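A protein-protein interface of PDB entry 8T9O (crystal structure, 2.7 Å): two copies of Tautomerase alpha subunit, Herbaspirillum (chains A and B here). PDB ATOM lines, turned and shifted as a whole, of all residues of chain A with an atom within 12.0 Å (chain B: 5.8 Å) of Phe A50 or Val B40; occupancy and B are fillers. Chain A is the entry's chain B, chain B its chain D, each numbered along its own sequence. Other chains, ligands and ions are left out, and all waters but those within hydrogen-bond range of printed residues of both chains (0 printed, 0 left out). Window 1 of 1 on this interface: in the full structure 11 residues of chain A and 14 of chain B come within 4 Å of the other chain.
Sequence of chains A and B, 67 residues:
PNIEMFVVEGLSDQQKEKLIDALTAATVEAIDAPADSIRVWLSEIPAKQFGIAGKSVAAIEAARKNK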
ATOM      1  N   GLU A   4      -9.976  -7.265 -24.813  1.00  0.00           N
ATOM      2  CA  GLU A   4      -9.011  -7.989 -23.997  1.00  0.00           C
ATOM      3  C   GLU A   4      -9.596  -8.153 -22.604  1.00  0.00           C
ATOM      4  O   GLU A   4      -9.953  -7.161 -21.961  1.00  0.00           O
ATOM      5  CB  GLU A   4      -7.679  -7.247 -23.912  1.00  0.00           C
ATOM      6  CG  GLU A   4      -6.670  -7.932 -23.001  1.00  0.00           C
ATOM      7  CD  GLU A   4      -5.294  -7.299 -23.060  1.00  0.00           C
ATOM      8  OE1 GLU A   4      -5.210  -6.079 -23.312  1.00  0.00           O
ATOM      9  OE2 GLU A   4      -4.296  -8.018 -22.844  1.00  0.00           O
ATOM     10  N   MET A   5      -9.694  -9.393 -22.136  1.00  0.00           N
ATOM     11  CA  MET A   5     -10.062  -9.663 -20.755  1.00  0.00           C
ATOM     12  C   MET A   5      -8.874 -10.266 -20.025  1.00  0.00           C
ATOM     13  O   MET A   5      -8.254 -11.215 -20.514  1.00  0.00           O
ATOM     14  CB  MET A   5     -11.272 -10.596 -20.654  1.00  0.00           C
ATOM     15  CG  MET A   5     -11.774 -10.732 -19.221  1.00  0.00           C
ATOM     16  SD  MET A   5     -13.298 -11.671 -19.034  1.00  0.00           S
ATOM     17  CE  MET A   5     -13.719 -11.271 -17.337  1.00  0.00           C
ATOM     18  N   PHE A   6      -8.555  -9.700 -18.866  1.00  0.00           N
ATOM     19  CA  PHE A   6      -7.542 -10.247 -17.976  1.00  0.00           C
ATOM     20  C   PHE A   6      -8.241 -11.170 -16.987  1.00  0.00           C
ATOM     21  O   PHE A   6      -9.117 -10.733 -16.236  1.00  0.00           O
ATOM     22  CB  PHE A   6      -6.794  -9.131 -17.250  1.00  0.00           C
ATOM     23  CG  PHE A   6      -5.923  -8.299 -18.152  1.00  0.00           C
ATOM     24  CD1 PHE A   6      -4.718  -8.789 -18.625  1.00  0.00           C
ATOM     25  CD2 PHE A   6      -6.320  -7.026 -18.531  1.00  0.00           C
ATOM     26  CE1 PHE A   6      -3.919  -8.025 -19.459  1.00  0.00           C
ATOM     27  CE2 PHE A   6      -5.527  -6.256 -19.364  1.00  0.00           C
ATOM     28  CZ  PHE A   6      -4.325  -6.755 -19.829  1.00  0.00           C
ATOM     29  N   VAL A   7      -7.868 -12.442 -17.004  1.00  0.00           N
ATOM     30  CA  VAL A   7      -8.485 -13.464 -16.169  1.00  0.00           C
ATOM     31  C   VAL A   7      -7.419 -14.185 -15.363  1.00  0.00           C
ATOM     32  O   VAL A   7      -6.284 -14.361 -15.815  1.00  0.00           O
ATOM     33  CB  VAL A   7      -9.307 -14.465 -17.011  1.00  0.00           C
ATOM     34  CG1 VAL A   7     -10.510 -13.778 -17.607  1.00  0.00           C
ATOM     35  CG2 VAL A   7      -8.441 -15.012 -18.140  1.00  0.00           C
ATOM     36  N   VAL A   8      -7.795 -14.584 -14.152  1.00  0.00           N
ATOM     37  CA  VAL A   8      -6.928 -15.412 -13.326  1.00  0.00           C
ATOM     38  C   VAL A   8      -6.980 -16.853 -13.828  1.00  0.00           C
ATOM     39  O   VAL A   8      -7.942 -17.284 -14.470  1.00  0.00           O
ATOM     40  CB  VAL A   8      -7.331 -15.311 -11.839  1.00  0.00           C
ATOM     41  CG1 VAL A   8      -6.390 -16.117 -10.936  1.00  0.00           C
ATOM     42  CG2 VAL A   8      -7.371 -13.860 -11.403  1.00  0.00           C
ATOM     43  N   GLU A   9      -5.919 -17.601 -13.546  1.00  0.00           N
ATOM     44  CA  GLU A   9      -5.805 -18.973 -14.005  1.00  0.00           C
ATOM     45  C   GLU A   9      -6.852 -19.861 -13.331  1.00  0.00           C
ATOM     46  O   GLU A   9      -7.490 -19.490 -12.344  1.00  0.00           O
ATOM     47  CB  GLU A   9      -4.403 -19.509 -13.736  1.00  0.00           C
ATOM     48  CG  GLU A   9      -3.838 -20.393 -14.832  1.00  0.00           C
ATOM     49  CD  GLU A   9      -2.365 -20.674 -14.633  1.00  0.00           C
ATOM     50  OE1 GLU A   9      -1.764 -21.359 -15.485  1.00  0.00           O
ATOM     51  OE2 GLU A   9      -1.803 -20.206 -13.617  1.00  0.00           O
ATOM     52  N   GLY A  10      -7.013 -21.064 -13.881  1.00  0.00           N
ATOM     53  CA  GLY A  10      -7.970 -22.029 -13.381  1.00  0.00           C
ATOM     54  C   GLY A  10      -9.198 -22.202 -14.245  1.00  0.00           C
ATOM     55  O   GLY A  10     -10.064 -23.012 -13.902  1.00  0.00           O
ATOM     56  N   LEU A  11      -9.303 -21.472 -15.346  1.00  0.00           N
ATOM     57  CA  LEU A  11     -10.465 -21.551 -16.209  1.00  0.00           C
ATOM     58  C   LEU A  11     -10.295 -22.629 -17.267  1.00  0.00           C
ATOM     59  O   LEU A  11      -9.215 -22.797 -17.837  1.00  0.00           O
ATOM     60  CB  LEU A  11     -10.738 -20.197 -16.871  1.00  0.00           C
ATOM     61  CG  LEU A  11     -11.174 -19.102 -15.901  1.00  0.00           C
ATOM     62  CD1 LEU A  11     -11.444 -17.802 -16.638  1.00  0.00           C
ATOM     63  CD2 LEU A  11     -12.404 -19.532 -15.101  1.00  0.00           C
ATOM     64  N   LEU A  19     -17.080 -17.750 -22.417  1.00  0.00           N
ATOM     65  CA  LEU A  19     -16.781 -16.355 -22.104  1.00  0.00           C
ATOM     66  C   LEU A  19     -16.606 -15.540 -23.380  1.00  0.00           C
ATOM     67  O   LEU A  19     -17.213 -14.473 -23.538  1.00  0.00           O
ATOM     68  CB  LEU A  19     -15.527 -16.267 -21.238  1.00  0.00           C
ATOM     69  CG  LEU A  19     -15.281 -14.954 -20.504  1.00  0.00           C
ATOM     70  CD1 LEU A  19     -16.497 -14.529 -19.687  1.00  0.00           C
ATOM     71  CD2 LEU A  19     -14.048 -15.075 -19.628  1.00  0.00           C
ATOM     72  N   LEU A  42      -8.437 -13.596 -24.459  1.00  0.00           N
ATOM     73  CA  LEU A  42      -8.227 -13.667 -23.020  1.00  0.00           C
ATOM     74  C   LEU A  42      -6.733 -13.728 -22.736  1.00  0.00           C
ATOM     75  O   LEU A  42      -6.026 -14.585 -23.275  1.00  0.00           O
ATOM     76  CB  LEU A  42      -8.933 -14.888 -22.427  1.00  0.00           C
ATOM     77  CG  LEU A  42     -10.402 -15.059 -22.822  1.00  0.00           C
ATOM     78  CD1 LEU A  42     -10.964 -16.376 -22.301  1.00  0.00           C
ATOM     79  CD2 LEU A  42     -11.220 -13.881 -22.321  1.00  0.00           C
ATOM     80  N   SER A  43      -6.258 -12.812 -21.902  1.00  0.00           N
ATOM     81  CA  SER A  43      -4.847 -12.714 -21.545  1.00  0.00           C
ATOM     82  C   SER A  43      -4.740 -13.177 -20.093  1.00  0.00           C
ATOM     83  O   SER A  43      -5.028 -12.417 -19.165  1.00  0.00           O
ATOM     84  CB  SER A  43      -4.341 -11.290 -21.759  1.00  0.00           C
ATOM     85  OG  SER A  43      -2.929 -11.211 -21.678  1.00  0.00           O
ATOM     86  N   GLU A  44      -4.337 -14.433 -19.906  1.00  0.00           N
ATOM     87  CA  GLU A  44      -4.490 -15.122 -18.630  1.00  0.00           C
ATOM     88  C   GLU A  44      -3.294 -14.885 -17.715  1.00  0.00           C
ATOM     89  O   GLU A  44      -2.141 -14.944 -18.151  1.00  0.00           O
ATOM     90  CB  GLU A  44      -4.685 -16.621 -18.861  1.00  0.00           C
ATOM     91  CG  GLU A  44      -5.546 -17.293 -17.806  1.00  0.00           C
ATOM     92  CD  GLU A  44      -5.662 -18.792 -18.007  1.00  0.00           C
ATOM     93  OE1 GLU A  44      -4.836 -19.367 -18.744  1.00  0.00           O
ATOM     94  OE2 GLU A  44      -6.587 -19.394 -17.423  1.00  0.00           O
ATOM     95  N   ILE A  45      -3.581 -14.651 -16.439  1.00  0.00           N
ATOM     96  CA  ILE A  45      -2.591 -14.228 -15.463  1.00  0.00           C
ATOM     97  C   ILE A  45      -2.540 -15.295 -14.349  1.00  0.00           C
ATOM     98  O   ILE A  45      -3.591 -15.671 -13.843  1.00  0.00           O
ATOM     99  CB  ILE A  45      -2.906 -12.858 -14.854  1.00  0.00           C
ATOM    100  CG1 ILE A  45      -3.150 -11.831 -15.963  1.00  0.00           C
ATOM    101  CG2 ILE A  45      -1.782 -12.399 -13.934  1.00  0.00           C
ATOM    102  CD1 ILE A  45      -1.958 -11.602 -16.856  1.00  0.00           C
ATOM    103  N   PRO A  46      -1.362 -15.776 -13.974  1.00  0.00           N
ATOM    104  CA  PRO A  46      -1.284 -16.664 -12.807  1.00  0.00           C
ATOM    105  C   PRO A  46      -1.717 -15.940 -11.542  1.00  0.00           C
ATOM    106  O   PRO A  46      -1.494 -14.736 -11.382  1.00  0.00           O
ATOM    107  CB  PRO A  46       0.200 -17.043 -12.754  1.00  0.00           C
ATOM    108  CG  PRO A  46       0.647 -16.940 -14.177  1.00  0.00           C
ATOM    109  CD  PRO A  46      -0.090 -15.737 -14.713  1.00  0.00           C
ATOM    110  N   ALA A  47      -2.349 -16.696 -10.637  1.00  0.00           N
ATOM    111  CA  ALA A  47      -2.860 -16.121  -9.393  1.00  0.00           C
ATOM    112  C   ALA A  47      -1.779 -15.383  -8.621  1.00  0.00           C
ATOM    113  O   ALA A  47      -2.071 -14.412  -7.914  1.00  0.00           O
ATOM    114  CB  ALA A  47      -3.462 -17.222  -8.518  1.00  0.00           C
ATOM    115  N   LYS A  48      -0.532 -15.827  -8.747  1.00  0.00           N
ATOM    116  CA  LYS A  48       0.582 -15.208  -8.045  1.00  0.00           C
ATOM    117  C   LYS A  48       1.058 -13.916  -8.688  1.00  0.00           C
ATOM    118  O   LYS A  48       1.922 -13.247  -8.115  1.00  0.00           O
ATOM    119  CB  LYS A  48       1.739 -16.206  -7.949  1.00  0.00           C
ATOM    120  CG  LYS A  48       2.348 -16.599  -9.287  1.00  0.00           C
ATOM    121  CD  LYS A  48       3.340 -17.737  -9.093  1.00  0.00           C
ATOM    122  CE  LYS A  48       4.030 -18.144 -10.393  1.00  0.00           C
ATOM    123  NZ  LYS A  48       3.151 -18.935 -11.309  1.00  0.00           N
ATOM    124  N   GLN A  49       0.532 -13.538  -9.849  1.00  0.00           N
ATOM    125  CA  GLN A  49       1.003 -12.323 -10.483  1.00  0.00           C
ATOM    126  C   GLN A  49      -0.128 -11.324 -10.633  1.00  0.00           C
ATOM    127  O   GLN A  49       0.088 -10.229 -11.167  1.00  0.00           O
ATOM    128  CB  GLN A  49       1.618 -12.643 -11.852  1.00  0.00           C
ATOM    129  CG  GLN A  49       2.625 -13.779 -11.785  1.00  0.00           C
ATOM    130  CD  GLN A  49       3.348 -14.012 -13.087  1.00  0.00           C
ATOM    131  OE1 GLN A  49       3.290 -13.189 -13.998  1.00  0.00           O
ATOM    132  NE2 GLN A  49       3.835 -15.236 -13.260  1.00  0.00           N
ATOM    133  N   PHE A  50      -1.327 -11.685 -10.187  1.00  0.00           N
ATOM    134  CA  PHE A  50      -2.492 -10.811 -10.160  1.00  0.00           C
ATOM    135  C   PHE A  50      -2.700 -10.361  -8.720  1.00  0.00           C
ATOM    136  O   PHE A  50      -3.013 -11.180  -7.850  1.00  0.00           O
ATOM    137  CB  PHE A  50      -3.724 -11.537 -10.696  1.00  0.00           C
ATOM    138  CG  PHE A  50      -4.860 -10.628 -11.024  1.00  0.00           C
ATOM    139  CD1 PHE A  50      -5.604 -10.040 -10.014  1.00  0.00           C
ATOM    140  CD2 PHE A  50      -5.174 -10.343 -12.339  1.00  0.00           C
ATOM    141  CE1 PHE A  50      -6.646  -9.194 -10.308  1.00  0.00           C
ATOM    142  CE2 PHE A  50      -6.217  -9.497 -12.639  1.00  0.00           C
ATOM    143  CZ  PHE A  50      -6.953  -8.923 -11.619  1.00  0.00           C
ATOM    144  N   GLY A  51      -2.536  -9.068  -8.474  1.00  0.00           N
ATOM    145  CA  GLY A  51      -2.541  -8.521  -7.126  1.00  0.00           C
ATOM    146  C   GLY A  51      -3.754  -7.642  -6.874  1.00  0.00           C
ATOM    147  O   GLY A  51      -4.177  -6.883  -7.750  1.00  0.00           O
ATOM    148  N   ILE A  52      -4.304  -7.763  -5.671  1.00  0.00           N
ATOM    149  CA  ILE A  52      -5.376  -6.905  -5.184  1.00  0.00           C
ATOM    150  C   ILE A  52      -4.908  -6.303  -3.867  1.00  0.00           C
ATOM    151  O   ILE A  52      -4.655  -7.036  -2.901  1.00  0.00           O
ATOM    152  CB  ILE A  52      -6.694  -7.675  -5.005  1.00  0.00           C
ATOM    153  CG1 ILE A  52      -6.908  -8.648  -6.168  1.00  0.00           C
ATOM    154  CG2 ILE A  52      -7.866  -6.714  -4.886  1.00  0.00           C
ATOM    155  CD1 ILE A  52      -8.141  -9.508  -6.024  1.00  0.00           C
ATOM    156  N   ALA A  53      -4.769  -4.975  -3.839  1.00  0.00           N
ATOM    157  CA  ALA A  53      -4.367  -4.236  -2.640  1.00  0.00           C
ATOM    158  C   ALA A  53      -2.979  -4.651  -2.155  1.00  0.00           C
ATOM    159  O   ALA A  53      -2.735  -4.781  -0.953  1.00  0.00           O
ATOM    160  CB  ALA A  53      -5.402  -4.387  -1.522  1.00  0.00           C
ATOM    161  N   GLY A  54      -2.057  -4.859  -3.098  1.00  0.00           N
ATOM    162  CA  GLY A  54      -0.672  -5.140  -2.781  1.00  0.00           C
ATOM    163  C   GLY A  54      -0.327  -6.601  -2.574  1.00  0.00           C
ATOM    164  O   GLY A  54       0.853  -6.916  -2.375  1.00  0.00           O
ATOM    165  N   LYS A  55      -1.309  -7.500  -2.619  1.00  0.00           N
ATOM    166  CA  LYS A  55      -1.115  -8.919  -2.349  1.00  0.00           C
ATOM    167  C   LYS A  55      -1.814  -9.730  -3.433  1.00  0.00           C
ATOM    168  O   LYS A  55      -2.887  -9.348  -3.910  1.00  0.00           O
ATOM    169  CB  LYS A  55      -1.628  -9.278  -0.930  1.00  0.00           C
ATOM    170  CG  LYS A  55      -1.573 -10.760  -0.493  1.00  0.00           C
ATOM    171  CD  LYS A  55      -0.171 -11.369  -0.376  1.00  0.00           C
ATOM    172  CE  LYS A  55       0.617 -10.881   0.833  1.00  0.00           C
ATOM    173  NZ  LYS A  55       1.916 -11.611   0.952  1.00  0.00           N
ATOM    174  N   SER A  56      -1.188 -10.835  -3.834  1.00  0.00           N
ATOM    175  CA  SER A  56      -1.656 -11.620  -4.967  1.00  0.00           C
ATOM    176  C   SER A  56      -2.956 -12.353  -4.631  1.00  0.00           C
ATOM    177  O   SER A  56      -3.406 -12.393  -3.483  1.00  0.00           O
ATOM    178  CB  SER A  56      -0.585 -12.620  -5.399  1.00  0.00           C
ATOM    179  OG  SER A  56      -0.455 -13.663  -4.448  1.00  0.00           O
ATOM    180  N   VAL A  57      -3.561 -12.947  -5.667  1.00  0.00           N
ATOM    181  CA  VAL A  57      -4.761 -13.759  -5.488  1.00  0.00           C
ATOM    182  C   VAL A  57      -4.479 -15.010  -4.665  1.00  0.00           C
ATOM    183  O   VAL A  57      -5.411 -15.627  -4.135  1.00  0.00           O
ATOM    184  CB  VAL A  57      -5.360 -14.061  -6.882  1.00  0.00           C
ATOM    185  CG1 VAL A  57      -6.499 -15.070  -6.813  1.00  0.00           C
ATOM    186  CG2 VAL A  57      -5.849 -12.770  -7.521  1.00  0.00           C
ATOM    187  N   ALA A  58      -3.208 -15.387  -4.518  1.00  0.00           N
ATOM    188  CA  ALA A  58      -2.825 -16.300  -3.450  1.00  0.00           C
ATOM    189  C   ALA A  58      -2.891 -15.544  -2.129  1.00  0.00           C
ATOM    190  O   ALA A  58      -1.931 -14.860  -1.755  1.00  0.00           O
ATOM    191  CB  ALA A  58      -1.427 -16.874  -3.690  1.00  0.00           C
ATOM    192  N   ALA A  59      -4.023 -15.655  -1.434  1.00  0.00           N
ATOM    193  CA  ALA A  59      -4.348 -14.829  -0.269  1.00  0.00           C
ATOM    194  C   ALA A  59      -4.425 -13.356  -0.659  1.00  0.00           C
ATOM    195  O   ALA A  59      -5.394 -12.921  -1.286  1.00  0.00           O
ATOM    196  CB  ALA A  59      -3.335 -15.034   0.857  1.00  0.00           C
ATOM    197  N   ASN B   2      -6.014   0.863 -12.074  1.00  0.00           N
ATOM    198  CA  ASN B   2      -5.507  -0.456 -12.422  1.00  0.00           C
ATOM    199  C   ASN B   2      -4.151  -0.288 -13.089  1.00  0.00           C
ATOM    200  O   ASN B   2      -3.943   0.658 -13.854  1.00  0.00           O
ATOM    201  CB  ASN B   2      -6.475  -1.187 -13.355  1.00  0.00           C
ATOM    202  CG  ASN B   2      -7.850  -1.366 -12.739  1.00  0.00           C
ATOM    203  OD1 ASN B   2      -8.018  -2.101 -11.768  1.00  0.00           O
ATOM    204  ND2 ASN B   2      -8.840  -0.681 -13.299  1.00  0.00           N
ATOM    205  N   ILE B   3      -3.219  -1.190 -12.784  1.00  0.00           N
ATOM    206  CA  ILE B   3      -1.871  -1.124 -13.333  1.00  0.00           C
ATOM    207  C   ILE B   3      -1.520  -2.460 -13.972  1.00  0.00           C
ATOM    208  O   ILE B   3      -1.843  -3.526 -13.437  1.00  0.00           O
ATOM    209  CB  ILE B   3      -0.821  -0.747 -12.266  1.00  0.00           C
ATOM    210  CG1 ILE B   3      -1.300   0.433 -11.419  1.00  0.00           C
ATOM    211  CG2 ILE B   3       0.503  -0.405 -12.923  1.00  0.00           C
ATOM    212  CD1 ILE B   3      -0.256   0.946 -10.451  1.00  0.00           C
ATOM    213  N   GLU B   4      -0.856  -2.392 -15.125  1.00  0.00           N
ATOM    214  CA  GLU B   4      -0.340  -3.555 -15.838  1.00  0.00           C
ATOM    215  C   GLU B   4       1.142  -3.334 -16.084  1.00  0.00           C
ATOM    216  O   GLU B   4       1.524  -2.335 -16.702  1.00  0.00           O
ATOM    217  CB  GLU B   4      -1.058  -3.759 -17.169  1.00  0.00           C
ATOM    218  CG  GLU B   4      -0.474  -4.874 -18.023  1.00  0.00           C
ATOM    219  CD  GLU B   4      -1.233  -5.077 -19.318  1.00  0.00           C
ATOM    220  OE1 GLU B   4      -1.023  -6.113 -19.981  1.00  0.00           O
ATOM    221  OE2 GLU B   4      -2.029  -4.185 -19.684  1.00  0.00           O
ATOM    222  N   LEU B  19       6.963  -7.140  -6.077  1.00  0.00           N
ATOM    223  CA  LEU B  19       6.725  -6.010  -6.971  1.00  0.00           C
ATOM    224  C   LEU B  19       5.318  -5.445  -6.798  1.00  0.00           C
ATOM    225  O   LEU B  19       5.122  -4.229  -6.880  1.00  0.00           O
ATOM    226  CB  LEU B  19       6.951  -6.437  -8.422  1.00  0.00           C
ATOM    227  CG  LEU B  19       7.063  -5.365  -9.509  1.00  0.00           C
ATOM    228  CD1 LEU B  19       8.062  -4.284  -9.131  1.00  0.00           C
ATOM    229  CD2 LEU B  19       7.444  -6.008 -10.831  1.00  0.00           C
ATOM    230  N   ILE B  20       4.326  -6.307  -6.546  1.00  0.00           N
ATOM    231  CA  ILE B  20       2.932  -5.854  -6.532  1.00  0.00           C
ATOM    232  C   ILE B  20       2.688  -4.855  -5.403  1.00  0.00           C
ATOM    233  O   ILE B  20       2.093  -3.792  -5.620  1.00  0.00           O
ATOM    234  CB  ILE B  20       1.966  -7.053  -6.459  1.00  0.00           C
ATOM    235  CG1 ILE B  20       2.015  -7.870  -7.759  1.00  0.00           C
ATOM    236  CG2 ILE B  20       0.557  -6.576  -6.140  1.00  0.00           C
ATOM    237  CD1 ILE B  20       1.317  -9.217  -7.678  1.00  0.00           C
ATOM    238  N   LEU B  23       4.445  -1.365  -6.216  1.00  0.00           N
ATOM    239  CA  LEU B  23       3.720  -0.552  -7.188  1.00  0.00           C
ATOM    240  C   LEU B  23       2.406  -0.043  -6.610  1.00  0.00           C
ATOM    241  O   LEU B  23       1.977   1.075  -6.915  1.00  0.00           O
ATOM    242  CB  LEU B  23       3.466  -1.363  -8.457  1.00  0.00           C
ATOM    243  CG  LEU B  23       4.683  -2.022  -9.111  1.00  0.00           C
ATOM    244  CD1 LEU B  23       4.241  -2.998 -10.191  1.00  0.00           C
ATOM    245  CD2 LEU B  23       5.630  -0.979  -9.680  1.00  0.00           C
ATOM    246  N   THR B  24       1.751  -0.850  -5.769  1.00  0.00           N
ATOM    247  CA  THR B  24       0.494  -0.422  -5.165  1.00  0.00           C
ATOM    248  C   THR B  24       0.722   0.713  -4.171  1.00  0.00           C
ATOM    249  O   THR B  24       0.012   1.721  -4.202  1.00  0.00           O
ATOM    250  CB  THR B  24      -0.197  -1.601  -4.477  1.00  0.00           C
ATOM    251  OG1 THR B  24      -0.735  -2.485  -5.467  1.00  0.00           O
ATOM    252  CG2 THR B  24      -1.332  -1.105  -3.589  1.00  0.00           C
ATOM    253  N   ILE B  38      -6.774  -0.371  -5.899  1.00  0.00           N
ATOM    254  CA  ILE B  38      -5.694  -0.611  -6.852  1.00  0.00           C
ATOM    255  C   ILE B  38      -5.490  -2.104  -7.058  1.00  0.00           C
ATOM    256  O   ILE B  38      -5.278  -2.861  -6.103  1.00  0.00           O
ATOM    257  CB  ILE B  38      -4.391   0.084  -6.425  1.00  0.00           C
ATOM    258  CG1 ILE B  38      -4.491   1.596  -6.669  1.00  0.00           C
ATOM    259  CG2 ILE B  38      -3.170  -0.570  -7.070  1.00  0.00           C
ATOM    260  CD1 ILE B  38      -5.039   2.372  -5.537  1.00  0.00           C
ATOM    261  N   ARG B  39      -5.582  -2.515  -8.317  1.00  0.00           N
ATOM    262  CA  ARG B  39      -5.285  -3.861  -8.763  1.00  0.00           C
ATOM    263  C   ARG B  39      -4.049  -3.805  -9.645  1.00  0.00           C
ATOM    264  O   ARG B  39      -3.926  -2.928 -10.505  1.00  0.00           O
ATOM    265  CB  ARG B  39      -6.477  -4.449  -9.518  1.00  0.00           C
ATOM    266  CG  ARG B  39      -7.642  -4.683  -8.585  1.00  0.00           C
ATOM    267  CD  ARG B  39      -8.925  -5.048  -9.289  1.00  0.00           C
ATOM    268  NE  ARG B  39     -10.033  -5.040  -8.340  1.00  0.00           N
ATOM    269  CZ  ARG B  39     -10.494  -6.127  -7.728  1.00  0.00           C
ATOM    270  NH1 ARG B  39      -9.944  -7.308  -7.971  1.00  0.00           N
ATOM    271  NH2 ARG B  39     -11.502  -6.033  -6.873  1.00  0.00           N
ATOM    272  N   VAL B  40      -3.121  -4.718  -9.391  1.00  0.00           N
ATOM    273  CA  VAL B  40      -1.852  -4.780 -10.103  1.00  0.00           C
ATOM    274  C   VAL B  40      -1.672  -6.208 -10.586  1.00  0.00           C
ATOM    275  O   VAL B  40      -1.703  -7.147  -9.782  1.00  0.00           O
ATOM    276  CB  VAL B  40      -0.672  -4.352  -9.217  1.00  0.00           C
ATOM    277  CG1 VAL B  40       0.640  -4.768  -9.851  1.00  0.00           C
ATOM    278  CG2 VAL B  40      -0.705  -2.849  -8.984  1.00  0.00           C
ATOM    279  N   TRP B  41      -1.503  -6.377 -11.892  1.00  0.00           N
ATOM    280  CA  TRP B  41      -1.286  -7.690 -12.478  1.00  0.00           C
ATOM    281  C   TRP B  41      -0.080  -7.618 -13.399  1.00  0.00           C
ATOM    282  O   TRP B  41       0.023  -6.706 -14.226  1.00  0.00           O
ATOM    283  CB  TRP B  41      -2.536  -8.181 -13.222  1.00  0.00           C
ATOM    284  CG  TRP B  41      -2.846  -7.452 -14.492  1.00  0.00           C
ATOM    285  CD1 TRP B  41      -2.423  -7.779 -15.746  1.00  0.00           C
ATOM    286  CD2 TRP B  41      -3.655  -6.276 -14.634  1.00  0.00           C
ATOM    287  NE1 TRP B  41      -2.916  -6.879 -16.660  1.00  0.00           N
ATOM    288  CE2 TRP B  41      -3.676  -5.946 -16.002  1.00  0.00           C
ATOM    289  CE3 TRP B  41      -4.363  -5.471 -13.736  1.00  0.00           C
ATOM    290  CZ2 TRP B  41      -4.377  -4.844 -16.494  1.00  0.00           C
ATOM    291  CZ3 TRP B  41      -5.058  -4.377 -14.226  1.00  0.00           C
ATOM    292  CH2 TRP B  41      -5.060  -4.074 -15.592  1.00  0.00           C
ATOM    293  N   LEU B  42       0.837  -8.567 -13.239  1.00  0.00           N
ATOM    294  CA  LEU B  42       2.081  -8.581 -13.995  1.00  0.00           C
ATOM    295  C   LEU B  42       1.923  -9.448 -15.239  1.00  0.00           C
ATOM    296  O   LEU B  42       1.449 -10.585 -15.154  1.00  0.00           O
ATOM    297  CB  LEU B  42       3.230  -9.101 -13.130  1.00  0.00           C
ATOM    298  CG  LEU B  42       3.591  -8.308 -11.871  1.00  0.00           C
ATOM    299  CD1 LEU B  42       4.715  -8.990 -11.106  1.00  0.00           C
ATOM    300  CD2 LEU B  42       3.978  -6.887 -12.221  1.00  0.00           C
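O of Arg B39 is in hydrogen-bond range of N of Ile B3 (3.0 Å). The side-chain hydroxyl of Thr B24 sits at hydrogen-bond distance from the backbone carbonyl oxygen of Ile B20 (3.1 Å). O of Val A7 is in hydrogen-bond range of N of Ile A45, at 2.8 Å. The backbone carbonyl oxygen of Ile A45 is in hydrogen-bond range of the backbone NH of Glu A9, at 3.0 Å. The backbone NH (N) of Trp B41 lies close to the backbone carbonyl oxygen (O) of Ile B3, at 3.3 Å. The backbone carbonyl oxygen (O) of Phe A50 lies within hydrogen-bond range of the backbone NH (N) of Val A57 (2.9 Å).
Of the 12 printed residues of chain B, 8 touch a printed residue of chain A. Printed residues of chain A that touch a printed residue of chain B: Phe A6, Ile A45, Gln A49, Phe A50, Gly A51, Ile A52, Ala A53 and Gly A54. Among the printed residues, 16 pairs touch across the chains. Among the printed residues, no Asp or Glu carboxylate lies within 4 Å of a Lys or Arg side-chain nitrogen of the other chain.
Among the printed residues, merely in contact across the chains: Gln A49 with Trp B41 (3.2 Å), Phe A6 with Trp B41 (3.2 Å), Phe A6 with Glu B4 (3.4 Å), Gly A51 with Arg B39 (3.4 Å), Ile A52 with Arg B39 (3.4 Å), Phe A50 with Trp B41 (3.5 Å), Phe A50 with Val B40 (3.5 Å), Gly A54 with Thr B24 (3.6 Å), Gly A54 with Ile B20 (3.7 Å), Gly A51 with Ile B20 (3.8 Å), Gln A49 with Val B40 (3.8 Å), Gln A49 with Ile B20 (3.8 Å) and Ile A45 with Leu B42 (3.9 Å).
Positions printed for both chains: 4, 19 and 42.
Printed residues of chain B within 4 Å of Phe A6: Glu B4 (3.4 Å) and Trp B41 (3.2 Å). Of the printed residues of chain B, Ile A45 touches Leu B42. Phe A50 touches two residues of chain B. Printed residues of chain B within 4 Å of Gly A51: Ile B20 (3.8 Å), Arg B39 (3.4 Å) and Val B40 (2.5 Å). Printed residues of chain B within 4 Å of Ile A52: Arg B39. Of the printed residues of chain B, Ala A53 touches Ile B38 (3.1 Å). No residue of chain A comes within 4 Å of Ile B3. No residue of chain A comes within 4 Å of Leu B19. Ile B20 touches three residues of chain A. No residue of chain A comes within 4 Å of Leu B23. Of chain A, only Gly A54 comes within 4 Å of Thr B24. Of the printed residues of chain A, Arg B39 touches Gly A51 (3.4 Å) and Ile A52 (3.4 Å). Of chain A, only Gln A49 (3.8 Å), Phe A50 (3.5 Å) and Gly A51 (2.5 Å) come within 4 Å of Val B40. Printed residues of chain A within 4 Å of Leu B42: Ile A45 (3.9 Å) and Gln A49 (2.8 Å). The nearest residue of chain B that does not touch Phe A50 is Ile B20 (4.3 Å).
The backbone carbonyl oxygen of Gln A49 is in hydrogen-bond range of the backbone NH of Leu B42, at 2.8 Å. N of Gly A51 lies within hydrogen-bond range of O of Val B40 (2.5 Å). N of Ala A53 sits at hydrogen-bond distance from O of Ile B38 (3.1 Å).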
